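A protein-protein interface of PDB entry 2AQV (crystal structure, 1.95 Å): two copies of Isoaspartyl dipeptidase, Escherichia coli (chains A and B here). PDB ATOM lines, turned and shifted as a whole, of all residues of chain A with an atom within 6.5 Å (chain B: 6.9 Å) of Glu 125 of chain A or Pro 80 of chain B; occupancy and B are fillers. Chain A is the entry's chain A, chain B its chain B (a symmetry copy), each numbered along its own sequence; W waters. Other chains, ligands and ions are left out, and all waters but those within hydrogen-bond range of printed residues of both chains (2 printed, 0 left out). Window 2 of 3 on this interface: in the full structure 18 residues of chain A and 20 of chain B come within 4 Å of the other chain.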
ATOM      1  N   LEU A 117      14.668  -9.537 -33.328  1.00  0.00           N
ATOM      2  CA  LEU A 117      15.577 -10.099 -32.341  1.00  0.00           C
ATOM      3  C   LEU A 117      16.735  -9.163 -32.014  1.00  0.00           C
ATOM      4  O   LEU A 117      17.136  -8.991 -30.838  1.00  0.00           O
ATOM      5  CB  LEU A 117      16.048 -11.515 -32.771  1.00  0.00           C
ATOM      6  CG  LEU A 117      17.151 -12.120 -31.886  1.00  0.00           C
ATOM      7  CD1 LEU A 117      16.573 -12.565 -30.540  1.00  0.00           C
ATOM      8  CD2 LEU A 117      17.750 -13.340 -32.611  1.00  0.00           C
ATOM      9  N   ALA A 118      17.295  -8.548 -33.042  1.00  0.00           N
ATOM     10  CA  ALA A 118      18.404  -7.614 -32.801  1.00  0.00           C
ATOM     11  C   ALA A 118      17.992  -6.446 -31.917  1.00  0.00           C
ATOM     12  O   ALA A 118      18.707  -6.055 -30.994  1.00  0.00           O
ATOM     13  CB  ALA A 118      18.991  -7.048 -34.101  1.00  0.00           C
ATOM     14  N   LYS A 119      16.842  -5.869 -32.235  1.00  0.00           N
ATOM     15  CA  LYS A 119      16.312  -4.710 -31.479  1.00  0.00           C
ATOM     16  C   LYS A 119      16.064  -5.075 -30.012  1.00  0.00           C
ATOM     17  O   LYS A 119      16.339  -4.300 -29.059  1.00  0.00           O
ATOM     18  CB  LYS A 119      15.022  -4.219 -32.126  1.00  0.00           C
ATOM     19  CG  LYS A 119      14.406  -3.038 -31.365  1.00  0.00           C
ATOM     20  CD  LYS A 119      15.289  -1.782 -31.261  1.00  0.00           C
ATOM     21  CE  LYS A 119      14.466  -0.645 -30.684  1.00  0.00           C
ATOM     22  NZ  LYS A 119      15.103   0.645 -30.898  1.00  0.00           N
ATOM     23  N   THR A 120      15.532  -6.297 -29.824  1.00  0.00           N
ATOM     24  CA  THR A 120      15.290  -6.829 -28.462  1.00  0.00           C
ATOM     25  C   THR A 120      16.589  -6.855 -27.657  1.00  0.00           C
ATOM     26  O   THR A 120      16.692  -6.510 -26.470  1.00  0.00           O
ATOM     27  CB  THR A 120      14.671  -8.244 -28.564  1.00  0.00           C
ATOM     28  OG1 THR A 120      13.416  -8.147 -29.213  1.00  0.00           O
ATOM     29  CG2 THR A 120      14.396  -8.793 -27.190  1.00  0.00           C
ATOM     30  N   ARG A 121      17.632  -7.333 -28.327  1.00  0.00           N
ATOM     31  CA  ARG A 121      18.908  -7.427 -27.665  1.00  0.00           C
ATOM     32  C   ARG A 121      19.501  -6.055 -27.378  1.00  0.00           C
ATOM     33  O   ARG A 121      20.100  -5.836 -26.352  1.00  0.00           O
ATOM     34  CB  ARG A 121      19.864  -8.301 -28.459  1.00  0.00           C
ATOM     35  CG  ARG A 121      19.485  -9.765 -28.318  1.00  0.00           C
ATOM     36  CD  ARG A 121      20.284 -10.702 -29.217  1.00  0.00           C
ATOM     37  NE  ARG A 121      20.090 -12.116 -28.846  1.00  0.00           N
ATOM     38  CZ  ARG A 121      20.308 -13.117 -29.686  1.00  0.00           C
ATOM     39  NH1 ARG A 121      20.701 -12.883 -30.940  1.00  0.00           N
ATOM     40  NH2 ARG A 121      20.115 -14.363 -29.270  1.00  0.00           N
ATOM     41  N   ALA A 122      19.320  -5.105 -28.295  1.00  0.00           N
ATOM     42  CA  ALA A 122      19.855  -3.761 -28.081  1.00  0.00           C
ATOM     43  C   ALA A 122      19.269  -3.125 -26.810  1.00  0.00           C
ATOM     44  O   ALA A 122      19.950  -2.553 -25.956  1.00  0.00           O
ATOM     45  CB  ALA A 122      19.610  -2.893 -29.297  1.00  0.00           C
ATOM     46  N   LEU A 123      17.961  -3.293 -26.649  1.00  0.00           N
ATOM     47  CA  LEU A 123      17.216  -2.794 -25.498  1.00  0.00           C
ATOM     48  C   LEU A 123      17.696  -3.422 -24.184  1.00  0.00           C
ATOM     49  O   LEU A 123      17.849  -2.765 -23.145  1.00  0.00           O
ATOM     50  CB  LEU A 123      15.690  -2.931 -25.712  1.00  0.00           C
ATOM     51  CG  LEU A 123      15.136  -1.958 -26.757  1.00  0.00           C
ATOM     52  CD1 LEU A 123      13.665  -2.325 -27.019  1.00  0.00           C
ATOM     53  CD2 LEU A 123      15.271  -0.492 -26.268  1.00  0.00           C
ATOM     54  N   ASN A 124      17.992  -4.701 -24.203  1.00  0.00           N
ATOM     55  CA  ASN A 124      18.510  -5.302 -23.004  1.00  0.00           C
ATOM     56  C   ASN A 124      19.866  -4.667 -22.702  1.00  0.00           C
ATOM     57  O   ASN A 124      20.153  -4.315 -21.580  1.00  0.00           O
ATOM     58  CB  ASN A 124      18.700  -6.829 -23.145  1.00  0.00           C
ATOM     59  CG  ASN A 124      17.379  -7.565 -23.105  1.00  0.00           C
ATOM     60  OD1 ASN A 124      16.634  -7.433 -22.140  1.00  0.00           O
ATOM     61  ND2 ASN A 124      17.046  -8.242 -24.181  1.00  0.00           N
ATOM     62  N   GLU A 125      20.710  -4.524 -23.710  1.00  0.00           N
ATOM     63  CA  GLU A 125      22.003  -3.933 -23.498  1.00  0.00           C
ATOM     64  C   GLU A 125      21.835  -2.487 -23.051  1.00  0.00           C
ATOM     65  O   GLU A 125      22.585  -1.962 -22.224  1.00  0.00           O
ATOM     66  CB  GLU A 125      22.780  -3.956 -24.817  1.00  0.00           C
ATOM     67  CG  GLU A 125      24.144  -4.607 -24.687  1.00  0.00           C
ATOM     68  CD  GLU A 125      24.772  -4.576 -26.023  1.00  0.00           C
ATOM     69  OE1 GLU A 125      24.212  -5.060 -26.985  1.00  0.00           O
ATOM     70  OE2 GLU A 125      25.903  -3.903 -26.041  1.00  0.00           O
ATOM     71  N   GLU A 126      20.843  -1.823 -23.589  1.00  0.00           N
ATOM     72  CA  GLU A 126      20.645  -0.437 -23.198  1.00  0.00           C
ATOM     73  C   GLU A 126      20.125  -0.268 -21.752  1.00  0.00           C
ATOM     74  O   GLU A 126      20.166   0.811 -21.192  1.00  0.00           O
ATOM     75  CB  GLU A 126      19.831   0.355 -24.210  1.00  0.00           C
ATOM     76  CG  GLU A 126      20.679   0.562 -25.443  1.00  0.00           C
ATOM     77  CD  GLU A 126      19.903   1.216 -26.552  1.00  0.00           C
ATOM     78  OE1 GLU A 126      18.711   1.091 -26.700  1.00  0.00           O
ATOM     79  OE2 GLU A 126      20.631   1.949 -27.338  1.00  0.00           O
ATOM     80  N   GLY A 127      19.619  -1.297 -21.111  1.00  0.00           N
ATOM     81  CA  GLY A 127      19.225  -1.077 -19.740  1.00  0.00           C
ATOM     82  C   GLY A 127      17.919  -1.704 -19.296  1.00  0.00           C
ATOM     83  O   GLY A 127      17.715  -1.859 -18.092  1.00  0.00           O
ATOM     84  N   ILE A 128      17.020  -2.019 -20.224  1.00  0.00           N
ATOM     85  CA  ILE A 128      15.757  -2.623 -19.795  1.00  0.00           C
ATOM     86  C   ILE A 128      15.742  -4.114 -20.057  1.00  0.00           C
ATOM     87  O   ILE A 128      16.787  -4.713 -20.290  1.00  0.00           O
ATOM     88  CB  ILE A 128      14.513  -1.894 -20.278  1.00  0.00           C
ATOM     89  CG1 ILE A 128      14.481  -1.862 -21.809  1.00  0.00           C
ATOM     90  CG2 ILE A 128      14.506  -0.462 -19.736  1.00  0.00           C
ATOM     91  CD1 ILE A 128      13.041  -1.723 -22.292  1.00  0.00           C
ATOM     92  N   ARG A 371      16.708  -2.575 -13.478  1.00  0.00           N
ATOM     93  CA  ARG A 371      17.843  -3.344 -13.035  1.00  0.00           C
ATOM     94  C   ARG A 371      18.782  -2.530 -12.158  1.00  0.00           C
ATOM     95  O   ARG A 371      20.014  -2.559 -12.309  1.00  0.00           O
ATOM     96  CB  ARG A 371      18.559  -4.051 -14.175  1.00  0.00           C
ATOM     97  CG  ARG A 371      17.692  -5.161 -14.783  1.00  0.00           C
ATOM     98  CD  ARG A 371      18.450  -5.993 -15.815  1.00  0.00           C
ATOM     99  NE  ARG A 371      18.232  -5.540 -17.186  1.00  0.00           N
ATOM    100  CZ  ARG A 371      19.205  -5.103 -17.969  1.00  0.00           C
ATOM    101  NH1 ARG A 371      20.469  -5.086 -17.546  1.00  0.00           N
ATOM    102  NH2 ARG A 371      18.917  -4.696 -19.193  1.00  0.00           N
ATOM    103  N   LYS A 373      19.328   0.622 -12.077  1.00  0.00           N
ATOM    104  CA  LYS A 373      19.920   1.836 -12.616  1.00  0.00           C
ATOM    105  C   LYS A 373      18.901   2.949 -12.790  1.00  0.00           C
ATOM    106  O   LYS A 373      17.807   2.696 -13.274  1.00  0.00           O
ATOM    107  CB  LYS A 373      20.613   1.537 -13.928  1.00  0.00           C
ATOM    108  CG  LYS A 373      20.892   2.739 -14.812  1.00  0.00           C
ATOM    109  CD  LYS A 373      21.474   2.279 -16.156  1.00  0.00           C
ATOM    110  CE  LYS A 373      22.410   3.286 -16.789  1.00  0.00           C
ATOM    111  NZ  LYS A 373      22.999   2.793 -18.089  1.00  0.00           N
ATOM    112  N   GLY B  76      25.664  -1.521 -36.671  1.00  0.00           N
ATOM    113  CA  GLY B  76      25.558  -2.851 -36.088  1.00  0.00           C
ATOM    114  C   GLY B  76      26.918  -3.557 -35.900  1.00  0.00           C
ATOM    115  O   GLY B  76      26.962  -4.678 -35.399  1.00  0.00           O
ATOM    116  N   GLU B  77      28.050  -2.890 -36.294  1.00  0.00           N
ATOM    117  CA  GLU B  77      29.387  -3.497 -36.196  1.00  0.00           C
ATOM    118  C   GLU B  77      29.943  -3.651 -34.779  1.00  0.00           C
ATOM    119  O   GLU B  77      30.940  -4.309 -34.527  1.00  0.00           O
ATOM    120  CB  GLU B  77      30.431  -2.722 -37.042  1.00  0.00           C
ATOM    121  CG  GLU B  77      30.246  -2.892 -38.542  1.00  0.00           C
ATOM    122  CD  GLU B  77      29.737  -1.678 -39.244  1.00  0.00           C
ATOM    123  OE1 GLU B  77      28.889  -0.961 -38.765  1.00  0.00           O
ATOM    124  OE2 GLU B  77      30.256  -1.528 -40.439  1.00  0.00           O
ATOM    125  N   ALA B  78      29.313  -2.988 -33.837  1.00  0.00           N
ATOM    126  CA  ALA B  78      29.722  -3.115 -32.456  1.00  0.00           C
ATOM    127  C   ALA B  78      28.525  -3.636 -31.680  1.00  0.00           C
ATOM    128  O   ALA B  78      28.224  -3.195 -30.568  1.00  0.00           O
ATOM    129  CB  ALA B  78      30.168  -1.774 -31.885  1.00  0.00           C
ATOM    130  N   GLY B  79      27.782  -4.533 -32.315  1.00  0.00           N
ATOM    131  CA  GLY B  79      26.616  -5.069 -31.654  1.00  0.00           C
ATOM    132  C   GLY B  79      25.388  -4.230 -31.989  1.00  0.00           C
ATOM    133  O   GLY B  79      25.476  -3.157 -32.551  1.00  0.00           O
ATOM    134  N   PRO B  80      24.256  -4.801 -31.562  1.00  0.00           N
ATOM    135  CA  PRO B  80      22.906  -4.340 -31.775  1.00  0.00           C
ATOM    136  C   PRO B  80      22.541  -2.951 -31.401  1.00  0.00           C
ATOM    137  O   PRO B  80      21.688  -2.345 -32.088  1.00  0.00           O
ATOM    138  CB  PRO B  80      21.939  -5.373 -31.230  1.00  0.00           C
ATOM    139  CG  PRO B  80      22.811  -6.452 -30.641  1.00  0.00           C
ATOM    140  CD  PRO B  80      24.279  -6.040 -30.758  1.00  0.00           C
ATOM    141  N   THR B  81      23.199  -2.439 -30.370  1.00  0.00           N
ATOM    142  CA  THR B  81      22.903  -1.063 -30.011  1.00  0.00           C
ATOM    143  C   THR B  81      23.461  -0.115 -31.086  1.00  0.00           C
ATOM    144  O   THR B  81      23.046   1.046 -31.166  1.00  0.00           O
ATOM    145  CB  THR B  81      23.466  -0.686 -28.635  1.00  0.00           C
ATOM    146  OG1 THR B  81      24.868  -0.695 -28.812  1.00  0.00           O
ATOM    147  CG2 THR B  81      23.064  -1.711 -27.554  1.00  0.00           C
ATOM    148  N   THR B  82      24.373  -0.596 -31.956  1.00  0.00           N
ATOM    149  CA  THR B  82      24.935   0.296 -32.982  1.00  0.00           C
ATOM    150  C   THR B  82      24.191   0.314 -34.293  1.00  0.00           C
ATOM    151  O   THR B  82      24.653   0.890 -35.295  1.00  0.00           O
ATOM    152  CB  THR B  82      26.431   0.084 -33.213  1.00  0.00           C
ATOM    153  OG1 THR B  82      26.647  -1.209 -33.760  1.00  0.00           O
ATOM    154  CG2 THR B  82      27.104   0.287 -31.866  1.00  0.00           C
ATOM    155  N   ARG B  83      23.010  -0.269 -34.289  1.00  0.00           N
ATOM    156  CA  ARG B  83      22.197  -0.229 -35.516  1.00  0.00           C
ATOM    157  C   ARG B  83      21.575   1.157 -35.665  1.00  0.00           C
ATOM    158  O   ARG B  83      20.806   1.606 -34.823  1.00  0.00           O
ATOM    159  CB  ARG B  83      21.121  -1.294 -35.460  1.00  0.00           C
ATOM    160  CG  ARG B  83      21.773  -2.674 -35.469  1.00  0.00           C
ATOM    161  CD  ARG B  83      20.728  -3.698 -35.093  1.00  0.00           C
ATOM    162  NE  ARG B  83      19.782  -3.996 -36.167  1.00  0.00           N
ATOM    163  CZ  ARG B  83      18.500  -3.634 -36.240  1.00  0.00           C
ATOM    164  NH1 ARG B  83      17.862  -2.928 -35.315  1.00  0.00           N
ATOM    165  NH2 ARG B  83      17.800  -4.050 -37.269  1.00  0.00           N
ATOM    166  N   THR B  84      21.901   1.873 -36.727  1.00  0.00           N
ATOM    167  CA  THR B  84      21.354   3.229 -36.857  1.00  0.00           C
ATOM    168  C   THR B  84      19.872   3.271 -37.289  1.00  0.00           C
ATOM    169  O   THR B  84      19.334   2.312 -37.801  1.00  0.00           O
ATOM    170  CB  THR B  84      22.277   4.101 -37.713  1.00  0.00           C
ATOM    171  OG1 THR B  84      22.291   3.518 -38.978  1.00  0.00           O
ATOM    172  CG2 THR B  84      23.719   3.985 -37.202  1.00  0.00           C
HETATM  173  O   HOH W   1      20.214   1.510 -30.414  1.00  0.00           O
HETATM  174  O   HOH W   2      25.705  -3.186 -28.996  1.00  0.00           O
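Among the printed residues, merely in contact across the chains: Ala 118 of chain A with Pro 80 of chain B, Ala 118 of chain A with Arg 83 of chain B, Ala 122 of chain A with Pro 80 of chain B, Ala 122 of chain A with Thr 81 of chain B, Glu 125 of chain A with Pro 80 of chain B, Glu 125 of chain A with Thr 81 of chain B and Glu 126 of chain A with Thr 81 of chain B.
Glu 125 of chain A touches two residues of chain B. Pro 80 of chain B touches just these residues of chain A: Ala 118, Ala 122 and Glu 125. Printed residues of chain A within 4 Å of Thr 81 of chain B: Ala 122, Glu 125 and Glu 126. Printed residues of chain B within 4 Å of Glu 126 of chain A: Thr 81 (3.9 Å). Leu 123 of chain A touches none of the printed residues of chain B. The nearest residue of chain B that does not touch Glu 125 of chain A is Ala 78 of chain B (5.1 Å). The nearest printed residue of chain B that does not touch Ala 122 of chain A is Thr 82 of chain B (5.9 Å).
Of the 14 printed residues of chain A, 4 touch a printed residue of chain B. Printed residues of chain A that touch a printed residue of chain B: Ala 118, Ala 122, Glu 125 and Glu 126. Hydrophobic or aromatic side chains of chain A within 4 Å of the printed part of chain B: Ala 118 and Ala 122. Hydrophobic or aromatic side chains of chain B within 4 Å of the printed part of chain A: Pro 80. Among the printed residues, 7 pairs touch across the chains. Among the printed residues, no Asp or Glu carboxylate lies within 4 Å of a Lys or Arg side-chain nitrogen of the other chain.
No position is printed for both chains.
Water W2 lies within hydrogen-bond range of OG1 of Thr 81 of chain B (2.6 Å), O of Ala 78 of chain B (3.0 Å) and OE2 of Glu 125 of chain A (3.0 Å). Water W1 lies within hydrogen-bond range of O of Thr 81 of chain B (3.0 Å) and OE2 of Glu 126 of chain A (3.1 Å).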
